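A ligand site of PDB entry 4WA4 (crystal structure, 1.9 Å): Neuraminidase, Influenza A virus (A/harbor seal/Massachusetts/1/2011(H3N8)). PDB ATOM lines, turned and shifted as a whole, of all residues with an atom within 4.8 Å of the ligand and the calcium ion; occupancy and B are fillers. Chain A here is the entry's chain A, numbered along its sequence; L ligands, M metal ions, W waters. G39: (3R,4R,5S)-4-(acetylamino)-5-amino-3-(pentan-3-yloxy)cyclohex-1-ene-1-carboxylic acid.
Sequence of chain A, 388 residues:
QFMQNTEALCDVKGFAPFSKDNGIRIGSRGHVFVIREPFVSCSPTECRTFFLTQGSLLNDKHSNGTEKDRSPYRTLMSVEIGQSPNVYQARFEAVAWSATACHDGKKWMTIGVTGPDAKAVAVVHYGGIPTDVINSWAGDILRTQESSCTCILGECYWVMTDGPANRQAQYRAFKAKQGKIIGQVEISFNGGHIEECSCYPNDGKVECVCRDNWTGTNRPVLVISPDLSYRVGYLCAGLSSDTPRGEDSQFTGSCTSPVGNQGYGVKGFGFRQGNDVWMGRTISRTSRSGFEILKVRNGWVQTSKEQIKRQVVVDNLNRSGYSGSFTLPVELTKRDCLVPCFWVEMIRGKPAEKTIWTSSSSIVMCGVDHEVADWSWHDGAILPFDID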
ATOM      1  N   ARG A  36      -4.439  -3.187  33.554  1.00  0.00           N
ATOM      2  CA  ARG A  36      -3.940  -2.621  32.330  1.00  0.00           C
ATOM      3  C   ARG A  36      -5.094  -1.747  31.832  1.00  0.00           C
ATOM      4  O   ARG A  36      -6.103  -1.554  32.578  1.00  0.00           O
ATOM      5  CB  ARG A  36      -3.394  -3.823  31.562  1.00  0.00           C
ATOM      6  CG  ARG A  36      -3.137  -3.952  30.201  1.00  0.00           C
ATOM      7  CD  ARG A  36      -1.707  -4.163  29.695  1.00  0.00           C
ATOM      8  NE  ARG A  36      -1.866  -3.138  28.671  1.00  0.00           N
ATOM      9  CZ  ARG A  36      -2.207  -3.318  27.391  1.00  0.00           C
ATOM     10  NH1 ARG A  36      -2.439  -2.213  26.695  1.00  0.00           N
ATOM     11  NH2 ARG A  36      -2.229  -4.552  26.802  1.00  0.00           N
ATOM     12  N   GLU A  37      -4.855  -1.029  30.739  1.00  0.00           N
ATOM     13  CA  GLU A  37      -5.861  -0.132  30.196  1.00  0.00           C
ATOM     14  C   GLU A  37      -6.349   0.966  31.199  1.00  0.00           C
ATOM     15  O   GLU A  37      -7.576   1.176  31.406  1.00  0.00           O
ATOM     16  CB  GLU A  37      -7.039  -0.953  29.653  1.00  0.00           C
ATOM     17  CG  GLU A  37      -6.754  -1.972  28.567  1.00  0.00           C
ATOM     18  CD  GLU A  37      -6.348  -3.395  29.047  1.00  0.00           C
ATOM     19  OE1 GLU A  37      -6.626  -3.777  30.218  1.00  0.00           O
ATOM     20  OE2 GLU A  37      -5.650  -4.172  28.299  1.00  0.00           O
ATOM     21  N   ARG A  70      -9.410 -11.381  28.747  1.00  0.00           N
ATOM     22  CA  ARG A  70     -10.829 -11.243  29.061  1.00  0.00           C
ATOM     23  C   ARG A  70     -11.468 -12.206  30.143  1.00  0.00           C
ATOM     24  O   ARG A  70     -12.501 -12.882  29.927  1.00  0.00           O
ATOM     25  CB  ARG A  70     -11.654 -11.268  27.800  1.00  0.00           C
ATOM     26  CG  ARG A  70     -11.304 -10.112  26.839  1.00  0.00           C
ATOM     27  CD  ARG A  70     -12.261 -10.142  25.658  1.00  0.00           C
ATOM     28  NE  ARG A  70     -12.024 -11.344  24.865  1.00  0.00           N
ATOM     29  CZ  ARG A  70     -10.927 -11.577  24.144  1.00  0.00           C
ATOM     30  NH1 ARG A  70      -9.976 -10.638  23.983  1.00  0.00           N
ATOM     31  NH2 ARG A  70     -10.799 -12.717  23.510  1.00  0.00           N
ATOM     32  N   ARG A  74     -12.003  -9.495  35.884  1.00  0.00           N
ATOM     33  CA  ARG A  74     -11.573  -8.132  35.586  1.00  0.00           C
ATOM     34  C   ARG A  74     -12.681  -7.204  35.949  1.00  0.00           C
ATOM     35  O   ARG A  74     -13.863  -7.443  35.605  1.00  0.00           O
ATOM     36  CB  ARG A  74     -11.214  -7.972  34.121  1.00  0.00           C
ATOM     37  CG  ARG A  74     -10.073  -8.847  33.703  1.00  0.00           C
ATOM     38  CD  ARG A  74      -9.397  -8.296  32.485  1.00  0.00           C
ATOM     39  NE  ARG A  74      -8.576  -7.161  32.877  1.00  0.00           N
ATOM     40  CZ  ARG A  74      -7.756  -6.486  32.080  1.00  0.00           C
ATOM     41  NH1 ARG A  74      -7.655  -6.749  30.817  1.00  0.00           N
ATOM     42  NH2 ARG A  74      -7.007  -5.450  32.566  1.00  0.00           N
ATOM     43  N   TRP A  97     -14.077  -6.264  31.282  1.00  0.00           N
ATOM     44  CA  TRP A  97     -12.842  -6.434  30.611  1.00  0.00           C
ATOM     45  C   TRP A  97     -12.563  -5.442  29.430  1.00  0.00           C
ATOM     46  O   TRP A  97     -11.528  -5.556  28.706  1.00  0.00           O
ATOM     47  CB  TRP A  97     -12.635  -7.890  30.230  1.00  0.00           C
ATOM     48  CG  TRP A  97     -13.771  -8.640  29.582  1.00  0.00           C
ATOM     49  CD1 TRP A  97     -14.495  -9.709  30.120  1.00  0.00           C
ATOM     50  CD2 TRP A  97     -14.350  -8.404  28.261  1.00  0.00           C
ATOM     51  NE1 TRP A  97     -15.435 -10.210  29.157  1.00  0.00           N
ATOM     52  CE2 TRP A  97     -15.359  -9.412  28.037  1.00  0.00           C
ATOM     53  CE3 TRP A  97     -14.126  -7.460  27.269  1.00  0.00           C
ATOM     54  CZ2 TRP A  97     -16.138  -9.413  26.888  1.00  0.00           C
ATOM     55  CZ3 TRP A  97     -14.862  -7.535  26.069  1.00  0.00           C
ATOM     56  CH2 TRP A  97     -15.859  -8.486  25.911  1.00  0.00           C
ATOM     57  N   SER A  98     -13.475  -4.501  29.216  1.00  0.00           N
ATOM     58  CA  SER A  98     -13.300  -3.320  28.375  1.00  0.00           C
ATOM     59  C   SER A  98     -14.242  -2.291  28.948  1.00  0.00           C
ATOM     60  O   SER A  98     -15.312  -2.629  29.519  1.00  0.00           O
ATOM     61  CB  SER A  98     -13.634  -3.631  26.907  1.00  0.00           C
ATOM     62  OG  SER A  98     -13.601  -2.542  26.011  1.00  0.00           O
ATOM     63  N   ILE A 141     -16.691 -10.310  20.440  1.00  0.00           N
ATOM     64  CA  ILE A 141     -16.069  -9.394  21.413  1.00  0.00           C
ATOM     65  C   ILE A 141     -16.483  -7.953  21.244  1.00  0.00           C
ATOM     66  O   ILE A 141     -15.680  -7.104  20.957  1.00  0.00           O
ATOM     67  CB  ILE A 141     -14.539  -9.449  21.368  1.00  0.00           C
ATOM     68  CG1 ILE A 141     -14.037 -10.887  21.253  1.00  0.00           C
ATOM     69  CG2 ILE A 141     -13.930  -8.981  22.685  1.00  0.00           C
ATOM     70  CD1 ILE A 141     -12.627 -11.068  20.830  1.00  0.00           C
ATOM     71  N   ARG A 143     -16.754  -4.443  22.421  1.00  0.00           N
ATOM     72  CA  ARG A 143     -15.663  -3.709  23.043  1.00  0.00           C
ATOM     73  C   ARG A 143     -15.709  -2.195  22.807  1.00  0.00           C
ATOM     74  O   ARG A 143     -16.452  -1.694  21.919  1.00  0.00           O
ATOM     75  CB  ARG A 143     -14.351  -4.360  22.626  1.00  0.00           C
ATOM     76  CG  ARG A 143     -14.081  -4.242  21.144  1.00  0.00           C
ATOM     77  CD  ARG A 143     -12.928  -5.154  20.807  1.00  0.00           C
ATOM     78  NE  ARG A 143     -12.579  -5.188  19.401  1.00  0.00           N
ATOM     79  CZ  ARG A 143     -13.074  -5.997  18.482  1.00  0.00           C
ATOM     80  NH1 ARG A 143     -12.543  -5.914  17.306  1.00  0.00           N
ATOM     81  NH2 ARG A 143     -14.026  -6.918  18.719  1.00  0.00           N
ATOM     82  N   GLU A 146     -11.623   2.178  26.070  1.00  0.00           N
ATOM     83  CA  GLU A 146     -10.563   2.196  27.101  1.00  0.00           C
ATOM     84  C   GLU A 146     -10.012   3.576  27.375  1.00  0.00           C
ATOM     85  O   GLU A 146      -8.853   3.656  27.670  1.00  0.00           O
ATOM     86  CB  GLU A 146      -9.398   1.242  26.789  1.00  0.00           C
ATOM     87  CG  GLU A 146      -9.778   0.047  26.016  1.00  0.00           C
ATOM     88  CD  GLU A 146     -10.565  -1.034  26.797  1.00  0.00           C
ATOM     89  OE1 GLU A 146     -10.935  -0.726  27.966  1.00  0.00           O
ATOM     90  OE2 GLU A 146     -10.766  -2.188  26.196  1.00  0.00           O
ATOM     91  N   ALA A 165     -10.784  -8.653  14.991  1.00  0.00           N
ATOM     92  CA  ALA A 165      -9.762  -7.667  15.464  1.00  0.00           C
ATOM     93  C   ALA A 165      -8.783  -7.381  14.416  1.00  0.00           C
ATOM     94  O   ALA A 165      -7.993  -6.443  14.569  1.00  0.00           O
ATOM     95  CB  ALA A 165      -9.046  -8.177  16.715  1.00  0.00           C
ATOM     96  N   GLU A 195     -10.925   0.769  16.454  1.00  0.00           N
ATOM     97  CA  GLU A 195     -10.797   0.186  17.766  1.00  0.00           C
ATOM     98  C   GLU A 195     -10.350   1.331  18.678  1.00  0.00           C
ATOM     99  O   GLU A 195      -9.585   2.233  18.303  1.00  0.00           O
ATOM    100  CB  GLU A 195      -9.622  -0.876  17.867  1.00  0.00           C
ATOM    101  CG  GLU A 195      -9.574  -2.034  16.902  1.00  0.00           C
ATOM    102  CD  GLU A 195     -10.601  -3.118  17.317  1.00  0.00           C
ATOM    103  OE1 GLU A 195     -10.615  -4.198  16.686  1.00  0.00           O
ATOM    104  OE2 GLU A 195     -11.401  -2.855  18.246  1.00  0.00           O
ATOM    105  N   GLU A 196     -10.766   1.222  19.905  1.00  0.00           N
ATOM    106  CA  GLU A 196     -10.115   1.973  21.034  1.00  0.00           C
ATOM    107  C   GLU A 196      -9.979   3.425  20.823  1.00  0.00           C
ATOM    108  O   GLU A 196      -8.860   3.997  20.948  1.00  0.00           O
ATOM    109  CB  GLU A 196      -8.799   1.297  21.300  1.00  0.00           C
ATOM    110  CG  GLU A 196      -8.967  -0.114  21.898  1.00  0.00           C
ATOM    111  CD  GLU A 196      -7.618  -0.832  22.096  1.00  0.00           C
ATOM    112  OE1 GLU A 196      -6.558  -0.368  21.521  1.00  0.00           O
ATOM    113  OE2 GLU A 196      -7.545  -1.862  22.844  1.00  0.00           O
ATOM    114  N   ARG A 211      -7.691   3.473  16.489  1.00  0.00           N
ATOM    115  CA  ARG A 211      -6.722   2.501  16.166  1.00  0.00           C
ATOM    116  C   ARG A 211      -7.283   1.630  15.047  1.00  0.00           C
ATOM    117  O   ARG A 211      -8.394   0.993  15.211  1.00  0.00           O
ATOM    118  CB  ARG A 211      -6.397   1.716  17.423  1.00  0.00           C
ATOM    119  CG  ARG A 211      -5.677   0.374  17.191  1.00  0.00           C
ATOM    120  CD  ARG A 211      -5.493  -0.391  18.469  1.00  0.00           C
ATOM    121  NE  ARG A 211      -4.953  -1.731  18.274  1.00  0.00           N
ATOM    122  CZ  ARG A 211      -4.545  -2.520  19.225  1.00  0.00           C
ATOM    123  NH1 ARG A 211      -4.658  -2.159  20.480  1.00  0.00           N
ATOM    124  NH2 ARG A 211      -4.010  -3.692  18.973  1.00  0.00           N
ATOM    125  N   ASP A 212      -6.547   1.524  13.921  1.00  0.00           N
ATOM    126  CA  ASP A 212      -6.822   0.604  12.824  1.00  0.00           C
ATOM    127  C   ASP A 212      -5.973  -0.625  13.050  1.00  0.00           C
ATOM    128  O   ASP A 212      -4.776  -0.560  13.068  1.00  0.00           O
ATOM    129  CB  ASP A 212      -6.616   1.254  11.432  1.00  0.00           C
ATOM    130  CG  ASP A 212      -6.776   0.284  10.253  1.00  0.00           C
ATOM    131  OD1 ASP A 212      -6.381  -0.906  10.388  1.00  0.00           O
ATOM    132  OD2 ASP A 212      -7.250   0.742   9.154  1.00  0.00           O
ATOM    133  N   ASN A 213      -6.597  -1.798  13.334  1.00  0.00           N
ATOM    134  CA  ASN A 213      -5.849  -2.987  13.698  1.00  0.00           C
ATOM    135  C   ASN A 213      -5.774  -3.975  12.498  1.00  0.00           C
ATOM    136  O   ASN A 213      -5.330  -5.092  12.640  1.00  0.00           O
ATOM    137  CB  ASN A 213      -6.465  -3.646  14.911  1.00  0.00           C
ATOM    138  CG  ASN A 213      -5.462  -4.374  15.759  1.00  0.00           C
ATOM    139  OD1 ASN A 213      -4.460  -3.790  16.196  1.00  0.00           O
ATOM    140  ND2 ASN A 213      -5.675  -5.623  16.003  1.00  0.00           N
ATOM    141  N   GLY A 216      -4.080  -0.440   8.495  1.00  0.00           N
ATOM    142  CA  GLY A 216      -3.610   0.946   8.556  1.00  0.00           C
ATOM    143  C   GLY A 216      -2.482   1.218   9.615  1.00  0.00           C
ATOM    144  O   GLY A 216      -2.514   0.720  10.758  1.00  0.00           O
ATOM    145  N   THR A 217      -1.510   2.047   9.194  1.00  0.00           N
ATOM    146  CA  THR A 217      -0.442   2.539  10.107  1.00  0.00           C
ATOM    147  C   THR A 217      -0.703   3.959  10.484  1.00  0.00           C
ATOM    148  O   THR A 217      -0.047   4.491  11.362  1.00  0.00           O
ATOM    149  CB  THR A 217       1.010   2.426   9.550  1.00  0.00           C
ATOM    150  OG1 THR A 217       1.078   3.200   8.397  1.00  0.00           O
ATOM    151  CG2 THR A 217       1.429   1.004   9.200  1.00  0.00           C
ATOM    152  N   ASP A 242       0.629   5.020  14.412  1.00  0.00           N
ATOM    153  CA  ASP A 242       0.375   3.732  14.979  1.00  0.00           C
ATOM    154  C   ASP A 242       1.645   3.016  15.270  1.00  0.00           C
ATOM    155  O   ASP A 242       2.741   3.497  14.850  1.00  0.00           O
ATOM    156  CB  ASP A 242      -0.529   2.885  14.024  1.00  0.00           C
ATOM    157  CG  ASP A 242      -1.381   1.814  14.820  1.00  0.00           C
ATOM    158  OD1 ASP A 242      -1.320   1.805  16.083  1.00  0.00           O
ATOM    159  OD2 ASP A 242      -2.128   1.028  14.206  1.00  0.00           O
ATOM    160  N   GLN A 262       0.170  -2.926   7.179  1.00  0.00           N
ATOM    161  CA  GLN A 262       0.708  -3.663   8.302  1.00  0.00           C
ATOM    162  C   GLN A 262      -0.469  -3.881   9.225  1.00  0.00           C
ATOM    163  O   GLN A 262      -1.383  -3.054   9.319  1.00  0.00           O
ATOM    164  CB  GLN A 262       1.770  -2.902   9.092  1.00  0.00           C
ATOM    165  CG  GLN A 262       3.093  -2.752   8.364  1.00  0.00           C
ATOM    166  CD  GLN A 262       4.203  -2.227   9.217  1.00  0.00           C
ATOM    167  OE1 GLN A 262       4.818  -1.225   8.927  1.00  0.00           O
ATOM    168  NE2 GLN A 262       4.504  -2.945  10.241  1.00  0.00           N
ATOM    169  N   GLY A 263      -0.415  -5.002   9.896  1.00  0.00           N
ATOM    170  CA  GLY A 263      -1.393  -5.356  10.922  1.00  0.00           C
ATOM    171  C   GLY A 263      -1.064  -4.786  12.290  1.00  0.00           C
ATOM    172  O   GLY A 263      -0.097  -4.008  12.491  1.00  0.00           O
ATOM    173  N   TYR A 264      -1.905  -5.170  13.232  1.00  0.00           N
ATOM    174  CA  TYR A 264      -1.745  -4.875  14.625  1.00  0.00           C
ATOM    175  C   TYR A 264      -1.855  -3.385  14.838  1.00  0.00           C
ATOM    176  O   TYR A 264      -2.316  -2.665  13.972  1.00  0.00           O
ATOM    177  CB  TYR A 264      -0.420  -5.422  15.234  1.00  0.00           C
ATOM    178  CG  TYR A 264      -0.523  -5.611  16.806  1.00  0.00           C
ATOM    179  CD1 TYR A 264      -1.652  -6.259  17.404  1.00  0.00           C
ATOM    180  CD2 TYR A 264       0.513  -5.137  17.699  1.00  0.00           C
ATOM    181  CE1 TYR A 264      -1.731  -6.481  18.801  1.00  0.00           C
ATOM    182  CE2 TYR A 264       0.402  -5.336  19.073  1.00  0.00           C
ATOM    183  CZ  TYR A 264      -0.710  -6.040  19.612  1.00  0.00           C
ATOM    184  OH  TYR A 264      -0.841  -6.271  20.982  1.00  0.00           O
ATOM    185  N   GLY A 265      -1.481  -2.883  16.012  1.00  0.00           N
ATOM    186  CA  GLY A 265      -1.708  -1.467  16.304  1.00  0.00           C
ATOM    187  C   GLY A 265      -1.590  -1.281  17.835  1.00  0.00           C
ATOM    188  O   GLY A 265      -1.205  -2.162  18.560  1.00  0.00           O
ATOM    189  N   ARG A 288       6.334  -1.174  21.648  1.00  0.00           N
ATOM    190  CA  ARG A 288       5.721  -0.141  22.424  1.00  0.00           C
ATOM    191  C   ARG A 288       6.750   0.399  23.376  1.00  0.00           C
ATOM    192  O   ARG A 288       6.744   0.081  24.595  1.00  0.00           O
ATOM    193  CB  ARG A 288       4.493  -0.734  23.132  1.00  0.00           C
ATOM    194  CG  ARG A 288       3.469  -1.180  22.115  1.00  0.00           C
ATOM    195  CD  ARG A 288       2.330  -1.983  22.756  1.00  0.00           C
ATOM    196  NE  ARG A 288       1.278  -2.324  21.844  1.00  0.00           N
ATOM    197  CZ  ARG A 288       0.130  -2.910  22.224  1.00  0.00           C
ATOM    198  NH1 ARG A 288      -0.856  -3.080  21.332  1.00  0.00           N
ATOM    199  NH2 ARG A 288      -0.051  -3.261  23.519  1.00  0.00           N
ATOM    200  N   TYR A 322      -0.466   1.960  25.715  1.00  0.00           N
ATOM    201  CA  TYR A 322      -1.586   2.762  25.280  1.00  0.00           C
ATOM    202  C   TYR A 322      -1.437   4.242  25.627  1.00  0.00           C
ATOM    203  O   TYR A 322      -0.738   4.629  26.574  1.00  0.00           O
ATOM    204  CB  TYR A 322      -2.879   2.214  25.942  1.00  0.00           C
ATOM    205  CG  TYR A 322      -3.507   0.976  25.267  1.00  0.00           C
ATOM    206  CD1 TYR A 322      -4.765   0.570  25.605  1.00  0.00           C
ATOM    207  CD2 TYR A 322      -2.832   0.255  24.293  1.00  0.00           C
ATOM    208  CE1 TYR A 322      -5.396  -0.505  24.965  1.00  0.00           C
ATOM    209  CE2 TYR A 322      -3.374  -0.872  23.686  1.00  0.00           C
ATOM    210  CZ  TYR A 322      -4.655  -1.284  24.031  1.00  0.00           C
ATOM    211  OH  TYR A 322      -5.302  -2.321  23.374  1.00  0.00           O
HETATM  212  C1  G39 L   1      -3.389  -4.838  23.140  1.00  0.00           C
HETATM  213  O1A G39 L   1      -3.096  -4.716  21.955  1.00  0.00           O
HETATM  214  O1B G39 L   1      -2.617  -4.495  24.047  1.00  0.00           O
HETATM  215  C2  G39 L   1      -4.759  -5.335  23.443  1.00  0.00           C
HETATM  216  C3  G39 L   1      -5.186  -5.656  24.866  1.00  0.00           C
HETATM  217  C4  G39 L   1      -6.668  -5.357  25.039  1.00  0.00           C
HETATM  218  C5  G39 L   1      -7.472  -6.131  24.005  1.00  0.00           C
HETATM  219  N5  G39 L   1      -8.905  -5.854  24.187  1.00  0.00           N
HETATM  220  C10 G39 L   1      -9.763  -6.799  24.581  1.00  0.00           C
HETATM  221  O10 G39 L   1      -9.392  -7.902  24.708  1.00  0.00           O
HETATM  222  C11 G39 L   1     -11.211  -6.435  24.826  1.00  0.00           C
HETATM  223  C6  G39 L   1      -7.137  -5.578  22.635  1.00  0.00           C
HETATM  224  C7  G39 L   1      -5.658  -5.383  22.412  1.00  0.00           C
HETATM  225  O7  G39 L   1      -7.628  -6.398  21.524  1.00  0.00           O
HETATM  226  C8  G39 L   1      -8.788  -5.765  20.970  1.00  0.00           C
HETATM  227  C9  G39 L   1      -8.563  -4.466  20.175  1.00  0.00           C
HETATM  228  C81 G39 L   1      -9.462  -6.803  20.093  1.00  0.00           C
HETATM  229  C82 G39 L   1     -10.059  -7.807  21.022  1.00  0.00           C
HETATM  230  C91 G39 L   1      -7.546  -4.584  19.089  1.00  0.00           C
HETATM  231  N4  G39 L   1      -7.097  -5.520  26.426  1.00  0.00           N
HETATM  232 CA    CA M   1      -2.425  -0.680  12.659  1.00  0.00          CA
HETATM  233  O   HOH W   1      -5.042  -6.516  29.076  1.00  0.00           O
HETATM  234  O   HOH W   2      -9.505  -2.990  24.074  1.00  0.00           O
HETATM  235  O   HOH W   3      -3.066  -2.529  11.092  1.00  0.00           O
HETATM  236  O   HOH W   4      -5.833  -7.907  26.592  1.00  0.00           O
HETATM  237  O   HOH W   5      -0.139  -1.090  12.432  1.00  0.00           O
HETATM  238  O   HOH W   6      -9.694  -4.213  27.176  1.00  0.00           O
HETATM  239  O   HOH W   7      -6.609  -8.623  20.904  1.00  0.00           O
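Water W3 lies within hydrogen-bond range of O of Gln 262 (2.5 Å) and N of Gly 216 (3.5 Å).
Water W2 lies within hydrogen-bond range of the side-chain carboxylate (OE2) of Glu 196, the side-chain carboxylate (OE2) of Glu 146 and a nitrogen (N5) of the ligand.
Water W6 lies within hydrogen-bond range of OE2 of Glu 146 (2.5 Å), O of Trp 97 (2.7 Å) and N4 of the ligand (3.0 Å).
Water W1 lies within hydrogen-bond range of the side-chain carboxylate (OE2) of Glu 37 (2.5 Å), the guanidinium group (NH1) of Arg 74 (3.1 Å) and a nitrogen (N4) of the ligand (3.5 Å).
The calcium ion is bound by the side-chain carboxylate of Asp 242 (2.3 Å), water W5 (2.3 Å), the backbone carbonyl oxygen of Gly 216 (2.4 Å), the backbone carbonyl oxygen of Tyr 264 (2.4 Å), the backbone carbonyl oxygen of Asp 212 (2.4 Å) and water W3 (2.5 Å).
The calcium ion has six donor atoms within binding distance.
Merely in contact with the calcium ion: Gly 265.
Of the 24 residues printed, 5 come within 4 Å of the calcium ion.
Along chain A the residues within 4 Å of the calcium ion span positions 212 to 265.
The side-chain carboxylate (OE1) of Glu 195 is in salt-bridge range of the guanidinium group (NH1) of Arg 143 (2.7 Å).
OE2 of Glu 37 is in salt-bridge range of NH2 of Arg 36 (3.8 Å).
The backbone carbonyl oxygen (O) of Gly 265 is in hydrogen-bond range of the guanidinium group (NH1) of Arg 288 (2.9 Å).
OH of Tyr 322 is in hydrogen-bond range of NH1 of Arg 211 (3.0 Å).
OH of Tyr 264 is in hydrogen-bond range of NH1 of Arg 288 (3.2 Å).
The backbone NH (N) of Gly 216 sits at hydrogen-bond distance from the side-chain carboxylate (OD1) of Asp 212 (3.0 Å).
The guanidinium group of Arg 143 lies within hydrogen-bond range of the backbone carbonyl oxygen of Ile 141.
The side-chain amide oxygen (OD1) of Asn 213 lies within hydrogen-bond range of the backbone NH (N) of Gly 265 (3.1 Å).
Merely in contact with the ligand: Tyr 322, Arg 143, Ala 165, Glu 196, Asn 213, Glu 195 and Trp 97.
Within 4 Å of the ligand: Arg 36, Glu 37, Arg 70, Trp 97, Arg 143, Ala 165, Glu 195, Glu 196, Arg 211, Asn 213, Tyr 264, Arg 288 and Tyr 322.
Along chain A the residues within 4 Å of the ligand span positions 36 to 322.
NH2 of Arg 211 lies within salt-bridge range of O1A of the ligand, at 3.3 Å.
NH2 of Arg 36 lies within salt-bridge range of O1B of the ligand (2.8 Å).
The guanidinium group (NH1) of Arg 288 is in salt-bridge range of an oxygen (O1A) of the ligand (2.8 Å).
NH1 of Arg 70 lies within hydrogen-bond range of O10 of the ligand, 2.9 Å away.
N4 of the ligand lies within salt-bridge range of OE2 of Glu 37 (2.7 Å).
O1A of the ligand sits at hydrogen-bond distance from OH of Tyr 264, 2.9 Å away.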
